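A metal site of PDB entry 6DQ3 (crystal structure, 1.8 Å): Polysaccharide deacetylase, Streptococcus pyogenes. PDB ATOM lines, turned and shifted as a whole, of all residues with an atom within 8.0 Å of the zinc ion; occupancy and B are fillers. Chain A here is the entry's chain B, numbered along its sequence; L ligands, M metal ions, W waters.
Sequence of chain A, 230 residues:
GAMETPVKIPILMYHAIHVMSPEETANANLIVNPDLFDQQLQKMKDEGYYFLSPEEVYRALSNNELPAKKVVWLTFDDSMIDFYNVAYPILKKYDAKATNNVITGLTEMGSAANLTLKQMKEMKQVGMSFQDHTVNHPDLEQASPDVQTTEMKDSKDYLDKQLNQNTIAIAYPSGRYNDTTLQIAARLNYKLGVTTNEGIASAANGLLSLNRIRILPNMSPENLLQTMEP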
ATOM      1  N   HIS A  15       5.535  20.516   0.003  1.00  0.00           N
ATOM      2  CA  HIS A  15       4.274  19.880  -0.354  1.00  0.00           C
ATOM      3  C   HIS A  15       4.124  19.918  -1.866  1.00  0.00           C
ATOM      4  O   HIS A  15       4.673  19.060  -2.574  1.00  0.00           O
ATOM      5  CB  HIS A  15       3.102  20.553   0.352  1.00  0.00           C
ATOM      6  CG  HIS A  15       2.875  20.041   1.745  1.00  0.00           C
ATOM      7  ND1 HIS A  15       3.646  20.432   2.814  1.00  0.00           N
ATOM      8  CD2 HIS A  15       1.968  19.147   2.223  1.00  0.00           C
ATOM      9  CE1 HIS A  15       3.217  19.815   3.907  1.00  0.00           C
ATOM     10  NE2 HIS A  15       2.199  19.031   3.580  1.00  0.00           N
ATOM     11  N   PHE A  76       8.737  15.429   1.616  1.00  0.00           N
ATOM     12  CA  PHE A  76       7.517  15.806   0.921  1.00  0.00           C
ATOM     13  C   PHE A  76       6.382  15.021   1.565  1.00  0.00           C
ATOM     14  O   PHE A  76       6.495  13.802   1.756  1.00  0.00           O
ATOM     15  CB  PHE A  76       7.597  15.449  -0.570  1.00  0.00           C
ATOM     16  CG  PHE A  76       8.545  16.315  -1.345  1.00  0.00           C
ATOM     17  CD1 PHE A  76       9.907  16.166  -1.204  1.00  0.00           C
ATOM     18  CD2 PHE A  76       8.058  17.245  -2.248  1.00  0.00           C
ATOM     19  CE1 PHE A  76      10.785  16.949  -1.936  1.00  0.00           C
ATOM     20  CE2 PHE A  76       8.926  18.029  -2.980  1.00  0.00           C
ATOM     21  CZ  PHE A  76      10.290  17.885  -2.817  1.00  0.00           C
ATOM     22  N   ASP A  77       5.280  15.701   1.859  1.00  0.00           N
ATOM     23  CA  ASP A  77       4.107  15.043   2.432  1.00  0.00           C
ATOM     24  C   ASP A  77       3.020  14.841   1.385  1.00  0.00           C
ATOM     25  O   ASP A  77       2.954  15.564   0.380  1.00  0.00           O
ATOM     26  CB  ASP A  77       3.547  15.853   3.602  1.00  0.00           C
ATOM     27  CG  ASP A  77       4.521  15.997   4.750  1.00  0.00           C
ATOM     28  OD1 ASP A  77       5.440  15.152   4.862  1.00  0.00           O
ATOM     29  OD2 ASP A  77       4.363  16.939   5.553  1.00  0.00           O
ATOM     30  N   ASP A  78       2.175  13.841   1.619  1.00  0.00           N
ATOM     31  CA  ASP A  78       0.881  13.594   0.967  1.00  0.00           C
ATOM     32  C   ASP A  78       0.967  12.854  -0.361  1.00  0.00           C
ATOM     33  O   ASP A  78      -0.059  12.729  -1.040  1.00  0.00           O
ATOM     34  CB  ASP A  78       0.101  14.903   0.740  1.00  0.00           C
ATOM     35  CG  ASP A  78      -0.333  15.560   2.035  1.00  0.00           C
ATOM     36  OD1 ASP A  78      -0.390  14.876   3.083  1.00  0.00           O
ATOM     37  OD2 ASP A  78      -0.629  16.771   2.031  1.00  0.00           O
ATOM     38  N   SER A  79       2.139  12.338  -0.729  1.00  0.00           N
ATOM     39  CA  SER A  79       2.330  11.491  -1.901  1.00  0.00           C
ATOM     40  C   SER A  79       1.487  11.941  -3.090  1.00  0.00           C
ATOM     41  O   SER A  79       0.712  11.185  -3.683  1.00  0.00           O
ATOM     42  CB  SER A  79       2.054  10.022  -1.547  1.00  0.00           C
ATOM     43  OG  SER A  79       0.885   9.882  -0.753  1.00  0.00           O
ATOM     44  N   MET A  80       1.694  13.207  -3.462  1.00  0.00           N
ATOM     45  CA  MET A  80       0.986  13.799  -4.589  1.00  0.00           C
ATOM     46  C   MET A  80       1.711  13.496  -5.895  1.00  0.00           C
ATOM     47  O   MET A  80       2.936  13.306  -5.926  1.00  0.00           O
ATOM     48  CB  MET A  80       0.843  15.297  -4.370  1.00  0.00           C
ATOM     49  CG  MET A  80       0.014  15.601  -3.134  1.00  0.00           C
ATOM     50  SD  MET A  80      -0.238  17.353  -2.779  1.00  0.00           S
ATOM     51  CE  MET A  80       1.385  17.825  -2.233  1.00  0.00           C
ATOM     52  N   ASN A 101       6.280  11.175   2.296  1.00  0.00           N
ATOM     53  CA  ASN A 101       5.470  10.537   3.330  1.00  0.00           C
ATOM     54  C   ASN A 101       4.099  10.223   2.746  1.00  0.00           C
ATOM     55  O   ASN A 101       3.330  11.136   2.431  1.00  0.00           O
ATOM     56  CB  ASN A 101       5.433  11.453   4.546  1.00  0.00           C
ATOM     57  CG  ASN A 101       6.834  11.706   5.105  1.00  0.00           C
ATOM     58  OD1 ASN A 101       7.577  10.765   5.382  1.00  0.00           O
ATOM     59  ND2 ASN A 101       7.209  12.975   5.215  1.00  0.00           N
ATOM     60  N   VAL A 102       3.792   8.933   2.640  1.00  0.00           N
ATOM     61  CA  VAL A 102       2.761   8.427   1.733  1.00  0.00           C
ATOM     62  C   VAL A 102       1.454   8.184   2.483  1.00  0.00           C
ATOM     63  O   VAL A 102       1.434   7.544   3.541  1.00  0.00           O
ATOM     64  CB  VAL A 102       3.230   7.129   1.042  1.00  0.00           C
ATOM     65  CG1 VAL A 102       2.153   6.598   0.099  1.00  0.00           C
ATOM     66  CG2 VAL A 102       4.554   7.341   0.324  1.00  0.00           C
ATOM     67  N   ILE A 103       0.356   8.662   1.893  1.00  0.00           N
ATOM     68  CA  ILE A 103      -1.003   8.316   2.331  1.00  0.00           C
ATOM     69  C   ILE A 103      -1.373   7.047   1.582  1.00  0.00           C
ATOM     70  O   ILE A 103      -1.766   7.091   0.406  1.00  0.00           O
ATOM     71  CB  ILE A 103      -1.993   9.453   2.045  1.00  0.00           C
ATOM     72  CG1 ILE A 103      -1.416  10.766   2.573  1.00  0.00           C
ATOM     73  CG2 ILE A 103      -3.351   9.172   2.684  1.00  0.00           C
ATOM     74  CD1 ILE A 103      -2.234  11.991   2.244  1.00  0.00           C
ATOM     75  N   HIS A 133       2.566   8.099   6.148  1.00  0.00           N
ATOM     76  CA  HIS A 133       1.676   9.245   6.357  1.00  0.00           C
ATOM     77  C   HIS A 133       0.248   8.765   6.619  1.00  0.00           C
ATOM     78  O   HIS A 133      -0.721   9.384   6.184  1.00  0.00           O
ATOM     79  CB  HIS A 133       1.742  10.194   5.158  1.00  0.00           C
ATOM     80  CG  HIS A 133       1.382  11.613   5.495  1.00  0.00           C
ATOM     81  ND1 HIS A 133       1.661  12.189   6.713  1.00  0.00           N
ATOM     82  CD2 HIS A 133       0.798  12.582   4.747  1.00  0.00           C
ATOM     83  CE1 HIS A 133       1.239  13.438   6.722  1.00  0.00           C
ATOM     84  NE2 HIS A 133       0.715  13.704   5.531  1.00  0.00           N
ATOM     85  N   THR A 134       0.129   7.634   7.321  1.00  0.00           N
ATOM     86  CA  THR A 134      -1.115   6.970   7.708  1.00  0.00           C
ATOM     87  C   THR A 134      -1.886   6.412   6.515  1.00  0.00           C
ATOM     88  O   THR A 134      -1.499   6.603   5.359  1.00  0.00           O
ATOM     89  CB  THR A 134      -2.052   7.910   8.496  1.00  0.00           C
ATOM     90  OG1 THR A 134      -2.725   8.802   7.607  1.00  0.00           O
ATOM     91  CG2 THR A 134      -1.277   8.703   9.541  1.00  0.00           C
ATOM     92  N   HIS A 137      -5.203   9.471   6.464  1.00  0.00           N
ATOM     93  CA  HIS A 137      -4.870  10.859   6.790  1.00  0.00           C
ATOM     94  C   HIS A 137      -5.852  11.477   7.777  1.00  0.00           C
ATOM     95  O   HIS A 137      -6.268  12.630   7.576  1.00  0.00           O
ATOM     96  CB  HIS A 137      -4.826  11.687   5.500  1.00  0.00           C
ATOM     97  CG  HIS A 137      -3.980  12.930   5.593  1.00  0.00           C
ATOM     98  ND1 HIS A 137      -4.497  14.163   5.939  1.00  0.00           N
ATOM     99  CD2 HIS A 137      -2.661  13.124   5.376  1.00  0.00           C
ATOM    100  CE1 HIS A 137      -3.533  15.057   5.934  1.00  0.00           C
ATOM    101  NE2 HIS A 137      -2.412  14.458   5.598  1.00  0.00           N
ATOM    102  N   PRO A 138      -6.223  10.783   8.850  1.00  0.00           N
ATOM    103  CA  PRO A 138      -7.036  11.424   9.891  1.00  0.00           C
ATOM    104  C   PRO A 138      -6.183  12.343  10.749  1.00  0.00           C
ATOM    105  O   PRO A 138      -4.952  12.348  10.683  1.00  0.00           O
ATOM    106  CB  PRO A 138      -7.552  10.231  10.709  1.00  0.00           C
ATOM    107  CG  PRO A 138      -6.410   9.244  10.627  1.00  0.00           C
ATOM    108  CD  PRO A 138      -5.883   9.387   9.198  1.00  0.00           C
ATOM    109  N   ALA A 171       5.241  10.887   9.253  1.00  0.00           N
ATOM    110  CA  ALA A 171       4.834  12.276   9.357  1.00  0.00           C
ATOM    111  C   ALA A 171       3.376  12.304   9.817  1.00  0.00           C
ATOM    112  O   ALA A 171       2.517  11.686   9.178  1.00  0.00           O
ATOM    113  CB  ALA A 171       4.982  13.009   8.010  1.00  0.00           C
ATOM    114  N   TYR A 172       3.100  13.003  10.923  1.00  0.00           N
ATOM    115  CA  TYR A 172       1.751  13.046  11.466  1.00  0.00           C
ATOM    116  C   TYR A 172       0.874  13.976  10.633  1.00  0.00           C
ATOM    117  O   TYR A 172       1.299  15.107  10.337  1.00  0.00           O
ATOM    118  CB  TYR A 172       1.763  13.489  12.926  1.00  0.00           C
ATOM    119  CG  TYR A 172       2.747  12.686  13.726  1.00  0.00           C
ATOM    120  CD1 TYR A 172       2.549  11.334  13.932  1.00  0.00           C
ATOM    121  CD2 TYR A 172       3.906  13.261  14.225  1.00  0.00           C
ATOM    122  CE1 TYR A 172       3.463  10.573  14.642  1.00  0.00           C
ATOM    123  CE2 TYR A 172       4.823  12.522  14.930  1.00  0.00           C
ATOM    124  CZ  TYR A 172       4.596  11.177  15.128  1.00  0.00           C
ATOM    125  OH  TYR A 172       5.511  10.428  15.831  1.00  0.00           O
ATOM    126  N   PRO A 173      -0.320  13.551  10.223  1.00  0.00           N
ATOM    127  CA  PRO A 173      -1.182  14.428   9.428  1.00  0.00           C
ATOM    128  C   PRO A 173      -1.423  15.765  10.114  1.00  0.00           C
ATOM    129  O   PRO A 173      -1.835  15.825  11.280  1.00  0.00           O
ATOM    130  CB  PRO A 173      -2.468  13.614   9.264  1.00  0.00           C
ATOM    131  CG  PRO A 173      -1.997  12.190   9.304  1.00  0.00           C
ATOM    132  CD  PRO A 173      -0.861  12.175  10.317  1.00  0.00           C
ATOM    133  N   SER A 174      -1.172  16.846   9.365  1.00  0.00           N
ATOM    134  CA  SER A 174      -1.319  18.227   9.813  1.00  0.00           C
ATOM    135  C   SER A 174      -0.460  18.536  11.035  1.00  0.00           C
ATOM    136  O   SER A 174      -0.675  19.551  11.702  1.00  0.00           O
ATOM    137  CB  SER A 174      -2.784  18.560  10.091  1.00  0.00           C
ATOM    138  OG  SER A 174      -3.573  18.373   8.917  1.00  0.00           O
ATOM    139  N   GLY A 175       0.522  17.701  11.324  1.00  0.00           N
ATOM    140  CA  GLY A 175       1.394  17.915  12.460  1.00  0.00           C
ATOM    141  C   GLY A 175       0.770  17.692  13.809  1.00  0.00           C
ATOM    142  O   GLY A 175       1.288  18.180  14.815  1.00  0.00           O
ATOM    143  N   THR A 196       5.101  19.535  12.154  1.00  0.00           N
ATOM    144  CA  THR A 196       5.102  20.827  11.464  1.00  0.00           C
ATOM    145  C   THR A 196       5.532  21.950  12.391  1.00  0.00           C
ATOM    146  O   THR A 196       5.296  23.132  12.090  1.00  0.00           O
ATOM    147  CB  THR A 196       3.726  21.131  10.867  1.00  0.00           C
ATOM    148  OG1 THR A 196       2.734  21.157  11.894  1.00  0.00           O
ATOM    149  CG2 THR A 196       3.351  20.090   9.824  1.00  0.00           C
ATOM    150  N   ARG A 212      10.610  20.628  11.556  1.00  0.00           N
ATOM    151  CA  ARG A 212      10.833  20.766  10.123  1.00  0.00           C
ATOM    152  C   ARG A 212      10.723  22.230   9.734  1.00  0.00           C
ATOM    153  O   ARG A 212      10.149  23.046  10.463  1.00  0.00           O
ATOM    154  CB  ARG A 212       9.842  19.930   9.308  1.00  0.00           C
ATOM    155  CG  ARG A 212      10.035  18.428   9.459  1.00  0.00           C
ATOM    156  CD  ARG A 212       9.300  17.652   8.366  1.00  0.00           C
ATOM    157  NE  ARG A 212       7.850  17.620   8.553  1.00  0.00           N
ATOM    158  CZ  ARG A 212       7.003  17.128   7.646  1.00  0.00           C
ATOM    159  NH1 ARG A 212       7.466  16.628   6.503  1.00  0.00           N
ATOM    160  NH2 ARG A 212       5.711  17.121   7.887  1.00  0.00           N
HETATM  161  C1  LIG L   1       0.833  17.226   6.460  1.00  0.00           C
HETATM  162  O1  LIG L   1       1.156  17.260   5.267  1.00  0.00           O
HETATM  163  O2  LIG L   1      -0.165  16.632   6.922  1.00  0.00           O
HETATM  164  C2  LIG L   1       1.696  17.898   7.391  1.00  0.00           C
HETATM  165 ZN    ZN M   1      -0.558  15.413   5.084  1.00  0.00          ZN
HETATM  166  O   HOH W   1      -1.736  17.402   4.363  1.00  0.00           O
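Within 4 Å of the zinc ion: Asp 78, His 133 and His 137. The nearest printed residue that does not touch the zinc ion is Asp 77 (4.4 Å).
The side-chain hydroxyl (OG1) of Thr 134 lies within hydrogen-bond range of the backbone NH (N) of His 137, at 2.8 Å. ND1 of His 133 is in hydrogen-bond range of O of Ala 171. The backbone carbonyl oxygen of Asn 101 sits at hydrogen-bond distance from the backbone NH of Asp 78, 3.1 Å away. The backbone NH (N) of His 133 sits at hydrogen-bond distance from the backbone carbonyl oxygen (O) of Val 102 (2.9 Å).
The zinc ion is bound by OD1 of Asp 78, NE2 of His 137, NE2 of His 133, O2 of the ligand, water W1 and O1 of the ligand. The zinc ion has six donor atoms within binding distance.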
